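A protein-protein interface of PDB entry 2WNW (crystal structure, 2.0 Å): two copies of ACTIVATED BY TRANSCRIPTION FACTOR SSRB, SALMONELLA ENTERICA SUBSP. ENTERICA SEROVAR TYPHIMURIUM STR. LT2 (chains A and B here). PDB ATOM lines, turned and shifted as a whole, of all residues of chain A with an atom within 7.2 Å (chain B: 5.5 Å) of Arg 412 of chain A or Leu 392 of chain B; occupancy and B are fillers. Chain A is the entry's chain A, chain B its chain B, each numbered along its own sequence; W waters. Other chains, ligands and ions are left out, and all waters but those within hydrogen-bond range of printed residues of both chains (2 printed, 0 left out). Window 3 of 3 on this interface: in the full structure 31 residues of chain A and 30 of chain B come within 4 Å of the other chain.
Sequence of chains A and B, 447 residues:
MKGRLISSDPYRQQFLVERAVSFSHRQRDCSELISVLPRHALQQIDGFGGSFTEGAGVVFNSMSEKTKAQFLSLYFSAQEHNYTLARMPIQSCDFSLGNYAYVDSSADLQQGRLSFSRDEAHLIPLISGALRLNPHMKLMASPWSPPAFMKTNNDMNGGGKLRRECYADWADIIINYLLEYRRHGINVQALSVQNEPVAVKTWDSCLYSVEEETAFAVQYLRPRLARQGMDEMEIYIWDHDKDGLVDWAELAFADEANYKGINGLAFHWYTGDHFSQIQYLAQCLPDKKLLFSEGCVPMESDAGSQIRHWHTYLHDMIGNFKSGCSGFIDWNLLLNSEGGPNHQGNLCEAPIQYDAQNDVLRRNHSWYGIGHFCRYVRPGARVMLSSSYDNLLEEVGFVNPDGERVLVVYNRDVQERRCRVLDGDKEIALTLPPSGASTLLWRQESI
Leu 392 of chain A touches Arg 412 of chain B, and with the chains exchanged Arg 412 of chain A touches Leu 392 of chain B. Arg 412 of chain A touches Asn 391 of chain B, but with the chains exchanged Asn 391 of chain A does not touch Arg 412 of chain B (4.5 Å).
OD2 of Asp 273 of chain A lies within hydrogen-bond range of N of Asn 391 of chain B. NH1 of Arg 412 of chain A sits close to ND2 of Asn 391 of chain B (3.1 Å).
Leu 392 of chain B touches just one residue of chain A: Arg 412 (3.6 Å). Printed residues of chain B within 4 Å of Asp 273 of chain A: Asp 390 (3.7 Å) and Asn 391 (3.0 Å). Printed residues of chain A within 4 Å of Asn 391 of chain B: Asp 273, His 315 and Arg 412. Printed residues of chain A within 4 Å of Asp 390 of chain B: Asp 273 (3.7 Å). Printed residues of chain B within 4 Å of His 315 of chain A: Asn 391. Of the printed residues of chain A, Arg 412 of chain B touches Leu 392. The nearest residue of chain B that does not touch Arg 412 of chain A is Asp 390 of chain B (5.0 Å). The nearest printed residue of chain B that does not touch His 315 of chain A is Asp 390 of chain B (5.6 Å).
Of the 18 printed residues of chain A, 4 touch a printed residue of chain B. Printed residues of chain A that touch a printed residue of chain B: Asp 273, His 315, Leu 392 and Arg 412. Hydrophobic or aromatic side chains of chain A within 4 Å of the printed part of chain B: His 315 and Leu 392. Of the 10 printed residues of chain B, 4 touch a printed residue of chain A. Among the printed residues, 6 pairs touch across the chains. Among the printed residues, no Asp or Glu carboxylate lies within 4 Å of a Lys or Arg side-chain nitrogen of the other chain.
Among the printed residues, pairs that only touch across the chains: His 315 of chain A with Asn 391 of chain B (3.1 Å), Arg 412 of chain A with Leu 392 of chain B (3.6 Å), Leu 392 of chain A with Arg 412 of chain B (3.7 Å) and Asp 273 of chain A with Asp 390 of chain B (3.7 Å).
Water W2 lies within hydrogen-bond range of the side-chain carboxylate of Asp 390 of chain B (2.5 Å), the side-chain amide nitrogen of Asn 391 of chain B (2.5 Å), the guanidinium group of Arg 412 of chain A (3.1 Å) and a ring nitrogen (NE2) of His 315 of chain A (3.5 Å). Water W1 bridges NH1 of Arg 412 of chain B and N of Asn 391 of chain A.
OE2 of Glu 394 of chain B is in salt-bridge range of NH1 of Arg 412 of chain B, at 3.7 Å. N of Arg 412 of chain A lies within hydrogen-bond range of O of Leu 392 of chain A, 3.1 Å away. OD2 of Asp 273 of chain A is in hydrogen-bond range of NE2 of His 315 of chain A (2.8 Å). N of Arg 412 of chain B sits at hydrogen-bond distance from O of Leu 392 of chain B (3.0 Å). The guanidinium group (NH1) of Arg 412 of chain A lies within salt-bridge range of the side-chain carboxylate (OE2) of Glu 394 of chain A, 3.8 Å away. The side-chain carboxylate of Asp 390 of chain B is in salt-bridge range of the guanidinium group of Arg 417 of chain B, 2.8 Å away.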
ATOM      1  N   ASP A 273      31.895   4.554  32.717  1.00  0.00           N
ATOM      2  CA  ASP A 273      31.787   6.007  32.832  1.00  0.00           C
ATOM      3  C   ASP A 273      31.615   6.574  34.242  1.00  0.00           C
ATOM      4  O   ASP A 273      32.532   7.194  34.782  1.00  0.00           O
ATOM      5  CB  ASP A 273      30.631   6.512  31.953  1.00  0.00           C
ATOM      6  CG  ASP A 273      30.790   6.137  30.483  1.00  0.00           C
ATOM      7  OD1 ASP A 273      31.856   5.603  30.102  1.00  0.00           O
ATOM      8  OD2 ASP A 273      29.840   6.386  29.700  1.00  0.00           O
ATOM      9  N   HIS A 311      37.689   5.282  20.714  1.00  0.00           N
ATOM     10  CA  HIS A 311      36.484   5.697  21.421  1.00  0.00           C
ATOM     11  C   HIS A 311      36.648   5.658  22.935  1.00  0.00           C
ATOM     12  O   HIS A 311      36.278   6.599  23.627  1.00  0.00           O
ATOM     13  CB  HIS A 311      35.302   4.799  21.059  1.00  0.00           C
ATOM     14  CG  HIS A 311      34.104   5.019  21.927  1.00  0.00           C
ATOM     15  ND1 HIS A 311      33.272   6.109  21.785  1.00  0.00           N
ATOM     16  CD2 HIS A 311      33.636   4.325  22.993  1.00  0.00           C
ATOM     17  CE1 HIS A 311      32.345   6.078  22.727  1.00  0.00           C
ATOM     18  NE2 HIS A 311      32.544   5.006  23.473  1.00  0.00           N
ATOM     19  N   HIS A 315      36.129   9.115  24.808  1.00  0.00           N
ATOM     20  CA  HIS A 315      34.880   9.151  25.560  1.00  0.00           C
ATOM     21  C   HIS A 315      35.112   9.355  27.054  1.00  0.00           C
ATOM     22  O   HIS A 315      34.442  10.173  27.684  1.00  0.00           O
ATOM     23  CB  HIS A 315      34.090   7.857  25.333  1.00  0.00           C
ATOM     24  CG  HIS A 315      32.798   7.795  26.089  1.00  0.00           C
ATOM     25  ND1 HIS A 315      31.699   8.556  25.753  1.00  0.00           N
ATOM     26  CD2 HIS A 315      32.435   7.070  27.175  1.00  0.00           C
ATOM     27  CE1 HIS A 315      30.716   8.305  26.600  1.00  0.00           C
ATOM     28  NE2 HIS A 315      31.136   7.407  27.473  1.00  0.00           N
ATOM     29  N   ASN A 391      24.209  15.050  22.498  1.00  0.00           N
ATOM     30  CA  ASN A 391      25.178  14.313  23.308  1.00  0.00           C
ATOM     31  C   ASN A 391      26.088  13.360  22.535  1.00  0.00           C
ATOM     32  O   ASN A 391      27.096  12.903  23.076  1.00  0.00           O
ATOM     33  CB  ASN A 391      24.459  13.530  24.415  1.00  0.00           C
ATOM     34  CG  ASN A 391      24.185  14.373  25.647  1.00  0.00           C
ATOM     35  OD1 ASN A 391      24.329  15.600  25.625  1.00  0.00           O
ATOM     36  ND2 ASN A 391      23.780  13.717  26.731  1.00  0.00           N
ATOM     37  N   LEU A 392      25.736  13.037  21.292  1.00  0.00           N
ATOM     38  CA  LEU A 392      26.569  12.147  20.487  1.00  0.00           C
ATOM     39  C   LEU A 392      27.788  12.931  20.018  1.00  0.00           C
ATOM     40  O   LEU A 392      28.813  12.356  19.658  1.00  0.00           O
ATOM     41  CB  LEU A 392      25.793  11.594  19.288  1.00  0.00           C
ATOM     42  CG  LEU A 392      24.663  10.611  19.611  1.00  0.00           C
ATOM     43  CD1 LEU A 392      24.079  10.077  18.314  1.00  0.00           C
ATOM     44  CD2 LEU A 392      25.192   9.458  20.459  1.00  0.00           C
ATOM     45  N   LEU A 393      27.658  14.254  20.001  1.00  0.00           N
ATOM     46  CA  LEU A 393      28.783  15.113  19.653  1.00  0.00           C
ATOM     47  C   LEU A 393      29.376  15.477  21.010  1.00  0.00           C
ATOM     48  O   LEU A 393      28.965  16.447  21.650  1.00  0.00           O
ATOM     49  CB  LEU A 393      28.313  16.369  18.907  1.00  0.00           C
ATOM     50  CG  LEU A 393      28.090  16.162  17.406  1.00  0.00           C
ATOM     51  CD1 LEU A 393      27.439  17.395  16.797  1.00  0.00           C
ATOM     52  CD2 LEU A 393      29.430  15.871  16.737  1.00  0.00           C
ATOM     53  N   GLU A 394      30.318  14.655  21.462  1.00  0.00           N
ATOM     54  CA  GLU A 394      30.972  14.848  22.748  1.00  0.00           C
ATOM     55  C   GLU A 394      31.945  16.007  22.658  1.00  0.00           C
ATOM     56  O   GLU A 394      32.677  16.138  21.680  1.00  0.00           O
ATOM     57  CB  GLU A 394      31.701  13.563  23.155  1.00  0.00           C
ATOM     58  CG  GLU A 394      30.763  12.367  23.327  1.00  0.00           C
ATOM     59  CD  GLU A 394      31.485  11.111  23.787  1.00  0.00           C
ATOM     60  OE1 GLU A 394      32.520  11.235  24.471  1.00  0.00           O
ATOM     61  OE2 GLU A 394      31.016  10.003  23.478  1.00  0.00           O
ATOM     62  N   TYR A 410      34.333  15.334  19.605  1.00  0.00           N
ATOM     63  CA  TYR A 410      34.416  13.959  19.127  1.00  0.00           C
ATOM     64  C   TYR A 410      33.026  13.477  18.713  1.00  0.00           C
ATOM     65  O   TYR A 410      32.077  13.528  19.502  1.00  0.00           O
ATOM     66  CB  TYR A 410      34.980  13.066  20.243  1.00  0.00           C
ATOM     67  CG  TYR A 410      34.711  11.584  20.072  1.00  0.00           C
ATOM     68  CD1 TYR A 410      34.112  10.849  21.098  1.00  0.00           C
ATOM     69  CD2 TYR A 410      35.041  10.921  18.890  1.00  0.00           C
ATOM     70  CE1 TYR A 410      33.845   9.490  20.948  1.00  0.00           C
ATOM     71  CE2 TYR A 410      34.780   9.561  18.730  1.00  0.00           C
ATOM     72  CZ  TYR A 410      34.181   8.855  19.762  1.00  0.00           C
ATOM     73  OH  TYR A 410      33.912   7.517  19.605  1.00  0.00           O
ATOM     74  N   ASN A 411      32.910  13.021  17.471  1.00  0.00           N
ATOM     75  CA  ASN A 411      31.639  12.532  16.946  1.00  0.00           C
ATOM     76  C   ASN A 411      31.548  11.011  17.076  1.00  0.00           C
ATOM     77  O   ASN A 411      32.157  10.283  16.290  1.00  0.00           O
ATOM     78  CB  ASN A 411      31.492  12.938  15.472  1.00  0.00           C
ATOM     79  CG  ASN A 411      30.272  12.318  14.820  1.00  0.00           C
ATOM     80  OD1 ASN A 411      29.304  11.985  15.503  1.00  0.00           O
ATOM     81  ND2 ASN A 411      30.306  12.169  13.493  1.00  0.00           N
ATOM     82  N   ARG A 412      30.783  10.528  18.055  1.00  0.00           N
ATOM     83  CA  ARG A 412      30.658   9.084  18.244  1.00  0.00           C
ATOM     84  C   ARG A 412      29.579   8.465  17.359  1.00  0.00           C
ATOM     85  O   ARG A 412      29.418   7.245  17.337  1.00  0.00           O
ATOM     86  CB  ARG A 412      30.377   8.741  19.718  1.00  0.00           C
ATOM     87  CG  ARG A 412      28.985   9.099  20.209  1.00  0.00           C
ATOM     88  CD  ARG A 412      28.768   8.653  21.652  1.00  0.00           C
ATOM     89  NE  ARG A 412      28.866   7.202  21.809  1.00  0.00           N
ATOM     90  CZ  ARG A 412      28.752   6.568  22.974  1.00  0.00           C
ATOM     91  NH1 ARG A 412      28.535   7.257  24.087  1.00  0.00           N
ATOM     92  NH2 ARG A 412      28.860   5.249  23.031  1.00  0.00           N
ATOM     93  N   ASP A 413      28.849   9.301  16.626  1.00  0.00           N
ATOM     94  CA  ASP A 413      27.794   8.814  15.741  1.00  0.00           C
ATOM     95  C   ASP A 413      28.459   8.030  14.610  1.00  0.00           C
ATOM     96  O   ASP A 413      29.656   8.189  14.355  1.00  0.00           O
ATOM     97  CB  ASP A 413      26.999   9.990  15.156  1.00  0.00           C
ATOM     98  CG  ASP A 413      25.577   9.605  14.746  1.00  0.00           C
ATOM     99  OD1 ASP A 413      25.283   8.395  14.622  1.00  0.00           O
ATOM    100  OD2 ASP A 413      24.751  10.523  14.545  1.00  0.00           O
ATOM    101  N   VAL A 414      27.681   7.191  13.935  1.00  0.00           N
ATOM    102  CA  VAL A 414      28.194   6.388  12.832  1.00  0.00           C
ATOM    103  C   VAL A 414      27.983   7.114  11.508  1.00  0.00           C
ATOM    104  O   VAL A 414      28.213   6.555  10.435  1.00  0.00           O
ATOM    105  CB  VAL A 414      27.487   5.020  12.766  1.00  0.00           C
ATOM    106  CG1 VAL A 414      27.796   4.214  14.025  1.00  0.00           C
ATOM    107  CG2 VAL A 414      25.990   5.222  12.615  1.00  0.00           C
ATOM    108  N   GLN A 415      27.529   8.360  11.595  1.00  0.00           N
ATOM    109  CA  GLN A 415      27.295   9.183  10.413  1.00  0.00           C
ATOM    110  C   GLN A 415      28.084  10.470  10.551  1.00  0.00           C
ATOM    111  O   GLN A 415      28.469  10.861  11.654  1.00  0.00           O
ATOM    112  CB  GLN A 415      25.827   9.585  10.293  1.00  0.00           C
ATOM    113  CG  GLN A 415      24.826   8.471  10.214  1.00  0.00           C
ATOM    114  CD  GLN A 415      23.421   9.025  10.133  1.00  0.00           C
ATOM    115  OE1 GLN A 415      23.120   9.840   9.257  1.00  0.00           O
ATOM    116  NE2 GLN A 415      22.555   8.599  11.046  1.00  0.00           N
ATOM    117  N   ARG A 417      28.594  14.227  11.008  1.00  0.00           N
ATOM    118  CA  ARG A 417      27.753  15.164  11.749  1.00  0.00           C
ATOM    119  C   ARG A 417      28.268  16.593  11.657  1.00  0.00           C
ATOM    120  O   ARG A 417      29.458  16.822  11.443  1.00  0.00           O
ATOM    121  CB  ARG A 417      27.654  14.748  13.222  1.00  0.00           C
ATOM    122  CG  ARG A 417      26.936  13.417  13.458  1.00  0.00           C
ATOM    123  CD  ARG A 417      25.493  13.464  12.967  1.00  0.00           C
ATOM    124  NE  ARG A 417      24.735  14.534  13.612  1.00  0.00           N
ATOM    125  CZ  ARG A 417      24.183  14.448  14.819  1.00  0.00           C
ATOM    126  NH1 ARG A 417      23.521  15.483  15.317  1.00  0.00           N
ATOM    127  NH2 ARG A 417      24.275  13.324  15.520  1.00  0.00           N
ATOM    128  N   PRO A 433      33.565  13.551  10.409  1.00  0.00           N
ATOM    129  CA  PRO A 433      33.189  12.250   9.859  1.00  0.00           C
ATOM    130  C   PRO A 433      32.871  11.332  11.034  1.00  0.00           C
ATOM    131  O   PRO A 433      33.099  11.696  12.194  1.00  0.00           O
ATOM    132  CB  PRO A 433      34.449  11.823   9.117  1.00  0.00           C
ATOM    133  CG  PRO A 433      35.539  12.387   9.985  1.00  0.00           C
ATOM    134  CD  PRO A 433      35.018  13.776  10.298  1.00  0.00           C
ATOM    135  N   PRO A 434      32.322  10.141  10.758  1.00  0.00           N
ATOM    136  CA  PRO A 434      32.004   9.216  11.852  1.00  0.00           C
ATOM    137  C   PRO A 434      33.281   8.949  12.653  1.00  0.00           C
ATOM    138  O   PRO A 434      34.338   8.703  12.070  1.00  0.00           O
ATOM    139  CB  PRO A 434      31.517   7.969  11.117  1.00  0.00           C
ATOM    140  CG  PRO A 434      30.923   8.528   9.856  1.00  0.00           C
ATOM    141  CD  PRO A 434      31.937   9.572   9.455  1.00  0.00           C
ATOM    142  N   SER A 435      33.178   9.006  13.980  1.00  0.00           N
ATOM    143  CA  SER A 435      34.310   8.780  14.879  1.00  0.00           C
ATOM    144  C   SER A 435      35.383   9.859  14.783  1.00  0.00           C
ATOM    145  O   SER A 435      36.431   9.765  15.421  1.00  0.00           O
ATOM    146  CB  SER A 435      34.943   7.405  14.627  1.00  0.00           C
ATOM    147  OG  SER A 435      34.052   6.364  14.990  1.00  0.00           O
ATOM    148  N   GLY A 436      35.120  10.899  14.003  1.00  0.00           N
ATOM    149  CA  GLY A 436      36.104  11.955  13.874  1.00  0.00           C
ATOM    150  C   GLY A 436      36.250  12.774  15.142  1.00  0.00           C
ATOM    151  O   GLY A 436      35.338  12.837  15.968  1.00  0.00           O
ATOM    152  N   ASP B 390      27.684   3.212  31.554  1.00  0.00           N
ATOM    153  CA  ASP B 390      27.663   3.463  30.111  1.00  0.00           C
ATOM    154  C   ASP B 390      26.564   4.491  29.857  1.00  0.00           C
ATOM    155  O   ASP B 390      25.383   4.197  30.042  1.00  0.00           O
ATOM    156  CB  ASP B 390      27.344   2.152  29.383  1.00  0.00           C
ATOM    157  CG  ASP B 390      27.482   2.258  27.880  1.00  0.00           C
ATOM    158  OD1 ASP B 390      27.284   3.363  27.335  1.00  0.00           O
ATOM    159  OD2 ASP B 390      27.776   1.224  27.241  1.00  0.00           O
ATOM    160  N   ASN B 391      26.932   5.692  29.423  1.00  0.00           N
ATOM    161  CA  ASN B 391      25.905   6.701  29.223  1.00  0.00           C
ATOM    162  C   ASN B 391      24.914   6.442  28.093  1.00  0.00           C
ATOM    163  O   ASN B 391      24.029   7.263  27.858  1.00  0.00           O
ATOM    164  CB  ASN B 391      26.518   8.107  29.116  1.00  0.00           C
ATOM    165  CG  ASN B 391      27.368   8.298  27.887  1.00  0.00           C
ATOM    166  OD1 ASN B 391      27.990   9.349  27.723  1.00  0.00           O
ATOM    167  ND2 ASN B 391      27.402   7.304  27.014  1.00  0.00           N
ATOM    168  N   LEU B 392      25.053   5.318  27.389  1.00  0.00           N
ATOM    169  CA  LEU B 392      24.068   4.982  26.360  1.00  0.00           C
ATOM    170  C   LEU B 392      22.866   4.455  27.143  1.00  0.00           C
ATOM    171  O   LEU B 392      21.744   4.398  26.639  1.00  0.00           O
ATOM    172  CB  LEU B 392      24.583   3.912  25.394  1.00  0.00           C
ATOM    173  CG  LEU B 392      25.594   4.400  24.350  1.00  0.00           C
ATOM    174  CD1 LEU B 392      25.829   3.308  23.326  1.00  0.00           C
ATOM    175  CD2 LEU B 392      25.070   5.661  23.666  1.00  0.00           C
ATOM    176  N   LEU B 393      23.129   4.055  28.386  1.00  0.00           N
ATOM    177  CA  LEU B 393      22.084   3.602  29.296  1.00  0.00           C
ATOM    178  C   LEU B 393      21.789   4.852  30.115  1.00  0.00           C
ATOM    179  O   LEU B 393      22.428   5.108  31.138  1.00  0.00           O
ATOM    180  CB  LEU B 393      22.588   2.475  30.206  1.00  0.00           C
ATOM    181  CG  LEU B 393      22.594   1.086  29.560  1.00  0.00           C
ATOM    182  CD1 LEU B 393      23.199   0.070  30.515  1.00  0.00           C
ATOM    183  CD2 LEU B 393      21.171   0.693  29.192  1.00  0.00           C
ATOM    184  N   GLU B 394      20.837   5.643  29.626  1.00  0.00           N
ATOM    185  CA  GLU B 394      20.447   6.890  30.260  1.00  0.00           C
ATOM    186  C   GLU B 394      19.582   6.626  31.476  1.00  0.00           C
ATOM    187  O   GLU B 394      18.677   5.797  31.442  1.00  0.00           O
ATOM    188  CB  GLU B 394      19.697   7.764  29.251  1.00  0.00           C
ATOM    189  CG  GLU B 394      20.548   8.182  28.058  1.00  0.00           C
ATOM    190  CD  GLU B 394      19.757   8.946  27.004  1.00  0.00           C
ATOM    191  OE1 GLU B 394      18.755   9.596  27.359  1.00  0.00           O
ATOM    192  OE2 GLU B 394      20.140   8.906  25.825  1.00  0.00           O
ATOM    193  N   TYR B 410      16.727   4.212  30.409  1.00  0.00           N
ATOM    194  CA  TYR B 410      16.424   4.183  28.982  1.00  0.00           C
ATOM    195  C   TYR B 410      17.657   3.719  28.200  1.00  0.00           C
ATOM    196  O   TYR B 410      18.736   4.303  28.322  1.00  0.00           O
ATOM    197  CB  TYR B 410      15.990   5.588  28.539  1.00  0.00           C
ATOM    198  CG  TYR B 410      15.951   5.800  27.043  1.00  0.00           C
ATOM    199  CD1 TYR B 410      16.645   6.858  26.459  1.00  0.00           C
ATOM    200  CD2 TYR B 410      15.233   4.941  26.210  1.00  0.00           C
ATOM    201  CE1 TYR B 410      16.630   7.057  25.080  1.00  0.00           C
ATOM    202  CE2 TYR B 410      15.211   5.129  24.830  1.00  0.00           C
ATOM    203  CZ  TYR B 410      15.916   6.192  24.273  1.00  0.00           C
ATOM    204  OH  TYR B 410      15.914   6.382  22.912  1.00  0.00           O
ATOM    205  N   ASN B 411      17.494   2.661  27.409  1.00  0.00           N
ATOM    206  CA  ASN B 411      18.594   2.110  26.618  1.00  0.00           C
ATOM    207  C   ASN B 411      18.581   2.646  25.196  1.00  0.00           C
ATOM    208  O   ASN B 411      17.813   2.174  24.367  1.00  0.00           O
ATOM    209  CB  ASN B 411      18.506   0.577  26.585  1.00  0.00           C
ATOM    210  CG  ASN B 411      19.525  -0.045  25.645  1.00  0.00           C
ATOM    211  OD1 ASN B 411      20.580   0.533  25.388  1.00  0.00           O
ATOM    212  ND2 ASN B 411      19.220  -1.235  25.137  1.00  0.00           N
ATOM    213  N   ARG B 412      19.439   3.615  24.899  1.00  0.00           N
ATOM    214  CA  ARG B 412      19.461   4.172  23.552  1.00  0.00           C
ATOM    215  C   ARG B 412      20.368   3.402  22.595  1.00  0.00           C
ATOM    216  O   ARG B 412      20.474   3.754  21.421  1.00  0.00           O
ATOM    217  CB  ARG B 412      19.861   5.654  23.582  1.00  0.00           C
ATOM    218  CG  ARG B 412      21.315   5.925  23.918  1.00  0.00           C
ATOM    219  CD  ARG B 412      21.634   7.417  23.783  1.00  0.00           C
ATOM    220  NE  ARG B 412      21.405   7.910  22.423  1.00  0.00           N
ATOM    221  CZ  ARG B 412      21.593   9.172  22.041  1.00  0.00           C
ATOM    222  NH1 ARG B 412      22.014  10.078  22.912  1.00  0.00           N
ATOM    223  NH2 ARG B 412      21.365   9.529  20.786  1.00  0.00           N
ATOM    224  N   ASP B 413      21.016   2.352  23.091  1.00  0.00           N
ATOM    225  CA  ASP B 413      21.889   1.542  22.246  1.00  0.00           C
ATOM    226  C   ASP B 413      21.000   0.784  21.257  1.00  0.00           C
ATOM    227  O   ASP B 413      19.792   0.648  21.473  1.00  0.00           O
ATOM    228  CB  ASP B 413      22.689   0.543  23.091  1.00  0.00           C
ATOM    229  CG  ASP B 413      23.971   0.085  22.411  1.00  0.00           C
ATOM    230  OD1 ASP B 413      24.076   0.212  21.174  1.00  0.00           O
ATOM    231  OD2 ASP B 413      24.877  -0.416  23.113  1.00  0.00           O
ATOM    232  N   ARG B 417      20.728  -4.480  26.160  1.00  0.00           N
ATOM    233  CA  ARG B 417      21.759  -4.140  27.137  1.00  0.00           C
ATOM    234  C   ARG B 417      21.386  -4.574  28.548  1.00  0.00           C
ATOM    235  O   ARG B 417      20.209  -4.668  28.897  1.00  0.00           O
ATOM    236  CB  ARG B 417      22.040  -2.629  27.131  1.00  0.00           C
ATOM    237  CG  ARG B 417      22.694  -2.110  25.850  1.00  0.00           C
ATOM    238  CD  ARG B 417      24.045  -2.777  25.598  1.00  0.00           C
ATOM    239  NE  ARG B 417      25.007  -2.516  26.668  1.00  0.00           N
ATOM    240  CZ  ARG B 417      25.735  -1.405  26.778  1.00  0.00           C
ATOM    241  NH1 ARG B 417      25.625  -0.434  25.876  1.00  0.00           N
ATOM    242  NH2 ARG B 417      26.562  -1.256  27.804  1.00  0.00           N
HETATM  243  O   HOH W   1      21.973  12.852  21.744  1.00  0.00           O
HETATM  244  O   HOH W   2      28.651   5.214  26.396  1.00  0.00           O
